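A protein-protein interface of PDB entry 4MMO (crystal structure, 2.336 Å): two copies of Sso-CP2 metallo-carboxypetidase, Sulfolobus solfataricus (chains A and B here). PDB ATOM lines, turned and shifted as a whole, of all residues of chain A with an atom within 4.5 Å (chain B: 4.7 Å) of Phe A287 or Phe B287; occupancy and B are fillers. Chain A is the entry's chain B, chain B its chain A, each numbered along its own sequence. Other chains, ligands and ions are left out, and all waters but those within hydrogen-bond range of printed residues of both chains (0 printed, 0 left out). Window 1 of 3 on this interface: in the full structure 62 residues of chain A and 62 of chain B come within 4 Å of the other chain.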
ATOM      1  N   CYS A 208      -9.156  26.436 -21.763  1.00  0.00           N
ATOM      2  CA  CYS A 208      -9.554  26.774 -20.395  1.00  0.00           C
ATOM      3  C   CYS A 208      -8.477  26.349 -19.413  1.00  0.00           C
ATOM      4  O   CYS A 208      -8.041  27.140 -18.575  1.00  0.00           O
ATOM      5  CB  CYS A 208     -10.874  26.106 -19.995  1.00  0.00           C
ATOM      6  SG  CYS A 208     -12.263  26.441 -21.074  1.00  0.00           S
ATOM      7  N   LEU A 211      -5.198  28.409 -19.939  1.00  0.00           N
ATOM      8  CA  LEU A 211      -5.206  29.757 -19.381  1.00  0.00           C
ATOM      9  C   LEU A 211      -5.277  29.719 -17.855  1.00  0.00           C
ATOM     10  O   LEU A 211      -4.748  30.602 -17.176  1.00  0.00           O
ATOM     11  CB  LEU A 211      -6.373  30.564 -19.943  1.00  0.00           C
ATOM     12  CG  LEU A 211      -6.387  32.053 -19.585  1.00  0.00           C
ATOM     13  CD1 LEU A 211      -5.110  32.754 -20.039  1.00  0.00           C
ATOM     14  CD2 LEU A 211      -7.600  32.722 -20.200  1.00  0.00           C
ATOM     15  N   ALA A 212      -5.933  28.694 -17.321  1.00  0.00           N
ATOM     16  CA  ALA A 212      -6.003  28.500 -15.879  1.00  0.00           C
ATOM     17  C   ALA A 212      -4.607  28.248 -15.330  1.00  0.00           C
ATOM     18  O   ALA A 212      -4.229  28.788 -14.290  1.00  0.00           O
ATOM     19  CB  ALA A 212      -6.928  27.330 -15.544  1.00  0.00           C
ATOM     20  N   ILE A 215      -2.443  31.513 -15.462  1.00  0.00           N
ATOM     21  CA  ILE A 215      -2.845  32.398 -14.374  1.00  0.00           C
ATOM     22  C   ILE A 215      -2.281  31.922 -13.039  1.00  0.00           C
ATOM     23  O   ILE A 215      -1.910  32.727 -12.184  1.00  0.00           O
ATOM     24  CB  ILE A 215      -4.388  32.473 -14.305  1.00  0.00           C
ATOM     25  CG1 ILE A 215      -4.898  33.523 -15.289  1.00  0.00           C
ATOM     26  CG2 ILE A 215      -4.877  32.792 -12.897  1.00  0.00           C
ATOM     27  CD1 ILE A 215      -6.396  33.491 -15.485  1.00  0.00           C
ATOM     28  N   GLY A 286     -11.713  38.726 -13.854  1.00  0.00           N
ATOM     29  CA  GLY A 286     -12.616  37.940 -14.669  1.00  0.00           C
ATOM     30  C   GLY A 286     -11.932  36.798 -15.390  1.00  0.00           C
ATOM     31  O   GLY A 286     -10.752  36.869 -15.726  1.00  0.00           O
ATOM     32  N   PHE A 287     -12.693  35.735 -15.609  1.00  0.00           N
ATOM     33  CA  PHE A 287     -12.251  34.600 -16.398  1.00  0.00           C
ATOM     34  C   PHE A 287     -13.514  33.966 -16.962  1.00  0.00           C
ATOM     35  O   PHE A 287     -14.426  33.606 -16.214  1.00  0.00           O
ATOM     36  CB  PHE A 287     -11.469  33.622 -15.517  1.00  0.00           C
ATOM     37  CG  PHE A 287     -10.770  32.514 -16.271  1.00  0.00           C
ATOM     38  CD1 PHE A 287     -11.392  31.832 -17.307  1.00  0.00           C
ATOM     39  CD2 PHE A 287      -9.484  32.143 -15.922  1.00  0.00           C
ATOM     40  CE1 PHE A 287     -10.743  30.814 -17.977  1.00  0.00           C
ATOM     41  CE2 PHE A 287      -8.831  31.125 -16.594  1.00  0.00           C
ATOM     42  CZ  PHE A 287      -9.461  30.461 -17.620  1.00  0.00           C
ATOM     43  N   GLU A 288     -13.567  33.853 -18.285  1.00  0.00           N
ATOM     44  CA  GLU A 288     -14.687  33.216 -18.963  1.00  0.00           C
ATOM     45  C   GLU A 288     -14.190  32.218 -20.003  1.00  0.00           C
ATOM     46  O   GLU A 288     -13.276  32.505 -20.780  1.00  0.00           O
ATOM     47  CB  GLU A 288     -15.566  34.264 -19.638  1.00  0.00           C
ATOM     48  CG  GLU A 288     -16.805  33.689 -20.309  1.00  0.00           C
ATOM     49  N   CYS A 289     -14.801  31.042 -20.012  1.00  0.00           N
ATOM     50  CA  CYS A 289     -14.514  30.046 -21.028  1.00  0.00           C
ATOM     51  C   CYS A 289     -15.625  29.013 -21.079  1.00  0.00           C
ATOM     52  O   CYS A 289     -16.082  28.533 -20.045  1.00  0.00           O
ATOM     53  CB  CYS A 289     -13.189  29.348 -20.742  1.00  0.00           C
ATOM     54  SG  CYS A 289     -12.728  28.172 -22.022  1.00  0.00           S
ATOM     55  N   THR A 292     -21.473  27.741 -19.418  1.00  0.00           N
ATOM     56  CA  THR A 292     -21.605  27.984 -17.987  1.00  0.00           C
ATOM     57  C   THR A 292     -23.054  28.277 -17.599  1.00  0.00           C
ATOM     58  O   THR A 292     -23.318  28.952 -16.604  1.00  0.00           O
ATOM     59  CB  THR A 292     -20.701  29.154 -17.556  1.00  0.00           C
ATOM     60  OG1 THR A 292     -21.107  30.356 -18.223  1.00  0.00           O
ATOM     61  CG2 THR A 292     -19.246  28.849 -17.907  1.00  0.00           C
ATOM     62  N   PHE A 305     -10.703  33.702 -22.098  1.00  0.00           N
ATOM     63  CA  PHE A 305     -10.040  34.942 -21.720  1.00  0.00           C
ATOM     64  C   PHE A 305     -10.123  35.246 -20.236  1.00  0.00           C
ATOM     65  O   PHE A 305     -10.966  34.714 -19.517  1.00  0.00           O
ATOM     66  CB  PHE A 305     -10.560  36.128 -22.534  1.00  0.00           C
ATOM     67  CG  PHE A 305     -12.000  36.454 -22.294  1.00  0.00           C
ATOM     68  CD1 PHE A 305     -12.366  37.360 -21.310  1.00  0.00           C
ATOM     69  CD2 PHE A 305     -12.990  35.875 -23.067  1.00  0.00           C
ATOM     70  CE1 PHE A 305     -13.695  37.671 -21.094  1.00  0.00           C
ATOM     71  CE2 PHE A 305     -14.321  36.185 -22.860  1.00  0.00           C
ATOM     72  CZ  PHE A 305     -14.674  37.083 -21.872  1.00  0.00           C
ATOM     73  N   ALA A 306      -9.218  36.109 -19.793  1.00  0.00           N
ATOM     74  CA  ALA A 306      -9.138  36.494 -18.400  1.00  0.00           C
ATOM     75  C   ALA A 306      -8.693  37.941 -18.308  1.00  0.00           C
ATOM     76  O   ALA A 306      -7.879  38.395 -19.110  1.00  0.00           O
ATOM     77  CB  ALA A 306      -8.163  35.599 -17.672  1.00  0.00           C
ATOM     78  N   CYS B 208     -11.459  33.152  -8.259  1.00  0.00           N
ATOM     79  CA  CYS B 208     -11.013  32.826  -9.619  1.00  0.00           C
ATOM     80  C   CYS B 208      -9.664  32.130  -9.599  1.00  0.00           C
ATOM     81  O   CYS B 208      -9.499  31.053 -10.172  1.00  0.00           O
ATOM     82  CB  CYS B 208     -10.883  34.081 -10.478  1.00  0.00           C
ATOM     83  SG  CYS B 208     -12.288  35.172 -10.422  1.00  0.00           S
ATOM     84  N   LEU B 211      -9.705  28.666  -7.762  1.00  0.00           N
ATOM     85  CA  LEU B 211     -10.315  27.616  -8.564  1.00  0.00           C
ATOM     86  C   LEU B 211      -9.447  27.276  -9.778  1.00  0.00           C
ATOM     87  O   LEU B 211      -9.315  26.105 -10.143  1.00  0.00           O
ATOM     88  CB  LEU B 211     -11.721  28.019  -9.008  1.00  0.00           C
ATOM     89  CG  LEU B 211     -12.546  26.918  -9.685  1.00  0.00           C
ATOM     90  CD1 LEU B 211     -12.660  25.673  -8.804  1.00  0.00           C
ATOM     91  CD2 LEU B 211     -13.930  27.436 -10.048  1.00  0.00           C
ATOM     92  N   ALA B 212      -8.853  28.296 -10.395  1.00  0.00           N
ATOM     93  CA  ALA B 212      -7.926  28.072 -11.503  1.00  0.00           C
ATOM     94  C   ALA B 212      -6.779  27.186 -11.043  1.00  0.00           C
ATOM     95  O   ALA B 212      -6.324  26.308 -11.775  1.00  0.00           O
ATOM     96  CB  ALA B 212      -7.388  29.396 -12.035  1.00  0.00           C
ATOM     97  N   ILE B 215      -8.154  23.371 -10.601  1.00  0.00           N
ATOM     98  CA  ILE B 215      -8.303  22.603 -11.832  1.00  0.00           C
ATOM     99  C   ILE B 215      -6.946  22.358 -12.491  1.00  0.00           C
ATOM    100  O   ILE B 215      -6.780  21.390 -13.231  1.00  0.00           O
ATOM    101  CB  ILE B 215      -9.284  23.269 -12.829  1.00  0.00           C
ATOM    102  CG1 ILE B 215      -8.816  24.674 -13.201  1.00  0.00           C
ATOM    103  CG2 ILE B 215     -10.689  23.301 -12.236  1.00  0.00           C
ATOM    104  CD1 ILE B 215      -9.682  25.355 -14.238  1.00  0.00           C
ATOM    105  N   VAL B 284     -12.288  20.336 -19.200  1.00  0.00           N
ATOM    106  CA  VAL B 284     -12.993  21.496 -18.666  1.00  0.00           C
ATOM    107  C   VAL B 284     -13.982  21.998 -19.711  1.00  0.00           C
ATOM    108  O   VAL B 284     -13.586  22.448 -20.786  1.00  0.00           O
ATOM    109  CB  VAL B 284     -12.019  22.630 -18.274  1.00  0.00           C
ATOM    110  CG1 VAL B 284     -12.782  23.852 -17.766  1.00  0.00           C
ATOM    111  CG2 VAL B 284     -11.033  22.147 -17.218  1.00  0.00           C
ATOM    112  N   ASP B 285     -15.270  21.913 -19.393  1.00  0.00           N
ATOM    113  CA  ASP B 285     -16.316  22.355 -20.308  1.00  0.00           C
ATOM    114  C   ASP B 285     -16.588  23.833 -20.124  1.00  0.00           C
ATOM    115  O   ASP B 285     -17.061  24.509 -21.039  1.00  0.00           O
ATOM    116  CB  ASP B 285     -17.613  21.584 -20.062  1.00  0.00           C
ATOM    117  CG  ASP B 285     -17.443  20.100 -20.218  1.00  0.00           C
ATOM    118  OD1 ASP B 285     -17.466  19.615 -21.369  1.00  0.00           O
ATOM    119  OD2 ASP B 285     -17.282  19.419 -19.189  1.00  0.00           O
ATOM    120  N   GLY B 286     -16.305  24.332 -18.929  1.00  0.00           N
ATOM    121  CA  GLY B 286     -16.618  25.707 -18.613  1.00  0.00           C
ATOM    122  C   GLY B 286     -15.922  26.219 -17.375  1.00  0.00           C
ATOM    123  O   GLY B 286     -15.649  25.475 -16.436  1.00  0.00           O
ATOM    124  N   PHE B 287     -15.622  27.509 -17.398  1.00  0.00           N
ATOM    125  CA  PHE B 287     -15.102  28.208 -16.240  1.00  0.00           C
ATOM    126  C   PHE B 287     -15.599  29.644 -16.309  1.00  0.00           C
ATOM    127  O   PHE B 287     -15.332  30.358 -17.277  1.00  0.00           O
ATOM    128  CB  PHE B 287     -13.573  28.157 -16.224  1.00  0.00           C
ATOM    129  CG  PHE B 287     -12.954  28.773 -14.996  1.00  0.00           C
ATOM    130  CD1 PHE B 287     -12.532  27.981 -13.942  1.00  0.00           C
ATOM    131  CD2 PHE B 287     -12.788  30.140 -14.903  1.00  0.00           C
ATOM    132  CE1 PHE B 287     -11.960  28.550 -12.816  1.00  0.00           C
ATOM    133  CE2 PHE B 287     -12.218  30.707 -13.784  1.00  0.00           C
ATOM    134  CZ  PHE B 287     -11.806  29.911 -12.741  1.00  0.00           C
ATOM    135  N   GLU B 288     -16.351  30.044 -15.289  1.00  0.00           N
ATOM    136  CA  GLU B 288     -16.906  31.387 -15.205  1.00  0.00           C
ATOM    137  C   GLU B 288     -16.516  32.014 -13.882  1.00  0.00           C
ATOM    138  O   GLU B 288     -16.594  31.378 -12.832  1.00  0.00           O
ATOM    139  CB  GLU B 288     -18.432  31.340 -15.306  1.00  0.00           C
ATOM    140  CG  GLU B 288     -19.130  32.687 -15.146  1.00  0.00           C
ATOM    141  CD  GLU B 288     -18.887  33.619 -16.318  1.00  0.00           C
ATOM    142  OE1 GLU B 288     -18.819  33.128 -17.466  1.00  0.00           O
ATOM    143  OE2 GLU B 288     -18.762  34.843 -16.094  1.00  0.00           O
ATOM    144  N   CYS B 289     -16.101  33.270 -13.939  1.00  0.00           N
ATOM    145  CA  CYS B 289     -15.816  34.023 -12.731  1.00  0.00           C
ATOM    146  C   CYS B 289     -15.691  35.507 -13.017  1.00  0.00           C
ATOM    147  O   CYS B 289     -15.138  35.909 -14.039  1.00  0.00           O
ATOM    148  CB  CYS B 289     -14.528  33.535 -12.084  1.00  0.00           C
ATOM    149  SG  CYS B 289     -14.167  34.425 -10.569  1.00  0.00           S
ATOM    150  N   PHE B 305     -17.094  29.252 -10.595  1.00  0.00           N
ATOM    151  CA  PHE B 305     -17.439  27.852 -10.817  1.00  0.00           C
ATOM    152  C   PHE B 305     -16.879  27.302 -12.123  1.00  0.00           C
ATOM    153  O   PHE B 305     -16.616  28.045 -13.072  1.00  0.00           O
ATOM    154  CB  PHE B 305     -18.957  27.635 -10.745  1.00  0.00           C
ATOM    155  CG  PHE B 305     -19.735  28.396 -11.776  1.00  0.00           C
ATOM    156  CD1 PHE B 305     -20.116  29.708 -11.546  1.00  0.00           C
ATOM    157  CD2 PHE B 305     -20.103  27.795 -12.967  1.00  0.00           C
ATOM    158  CE1 PHE B 305     -20.840  30.410 -12.493  1.00  0.00           C
ATOM    159  CE2 PHE B 305     -20.827  28.491 -13.917  1.00  0.00           C
ATOM    160  CZ  PHE B 305     -21.197  29.800 -13.679  1.00  0.00           C
ATOM    161  N   ALA B 306     -16.690  25.986 -12.141  1.00  0.00           N
ATOM    162  CA  ALA B 306     -16.170  25.286 -13.301  1.00  0.00           C
ATOM    163  C   ALA B 306     -16.949  23.991 -13.504  1.00  0.00           C
ATOM    164  O   ALA B 306     -17.461  23.414 -12.545  1.00  0.00           O
ATOM    165  CB  ALA B 306     -14.693  24.988 -13.110  1.00  0.00           C
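The backbone carbonyl oxygen (O) of Phe B287 is in hydrogen-bond range of the backbone NH (N) of Cys A289 (2.9 Å). The backbone NH (N) of Cys B289 is in hydrogen-bond range of the backbone carbonyl oxygen (O) of Phe A287, 2.8 Å away.
Among the printed residues, merely in contact across the chains: Cys A289 with Gly B286, Phe A287 with Phe B287, Gly A286 with Cys B289, Glu A288 with Phe B287, Phe A287 with Glu B288, Glu A288 with Glu B288, Ala A212 with Ile B215, Thr A292 with Glu B288, Thr A292 with Phe B305, Cys A208 with Val B284, Thr A292 with Phe B287 and Ala A212 with Ala B212.
The side-chain sulfur of Cys B208 forms a disulfide with the side-chain sulfur of Cys B289 (2.0 Å). N of Glu B288 sits at hydrogen-bond distance from O of Phe B305 (3.0 Å). SG of Cys A208 is disulfide-bonded to SG of Cys A289 (2.0 Å). N of Glu A288 sits at hydrogen-bond distance from O of Phe A305, 3.0 Å away.
Gly A286 touches Cys B289, and with the chains exchanged Cys A289 touches Gly B286. Phe B287 touches its own counterpart, Phe A287. Phe A287 touches Glu B288, and with the chains exchanged Glu A288 touches Phe B287. Phe A287 touches Cys B289, and with the chains exchanged Cys A289 touches Phe B287. Of the 14 pairs that touch across the chains among the printed residues, 9 have their exchanged pair printed and touching as well.
Printed residues of chain B within 4 Å of Cys A208: Val B284 (3.7 Å). Phe A305 touches none of the printed residues of chain B. Of the printed residues of chain A, Gly B286 touches Cys A289 (3.2 Å). Of chain A, only Phe A287 (3.3 Å), Glu A288 (3.4 Å), Cys A289 (2.9 Å) and Thr A292 (3.9 Å) come within 4 Å of Phe B287. Ala B306 touches none of the printed residues of chain A. The nearest printed residue of chain A that does not touch Phe B287 is Cys A208 (5.1 Å). The nearest printed residue of chain B that does not touch Gly A286 is Cys B208 (5.0 Å).
Of the 12 printed residues of chain B, 8 touch a printed residue of chain A. Among the printed residues, 14 pairs touch across the chains. Among the printed residues, no Asp or Glu carboxylate lies within 4 Å of a Lys or Arg side-chain nitrogen of the other chain.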
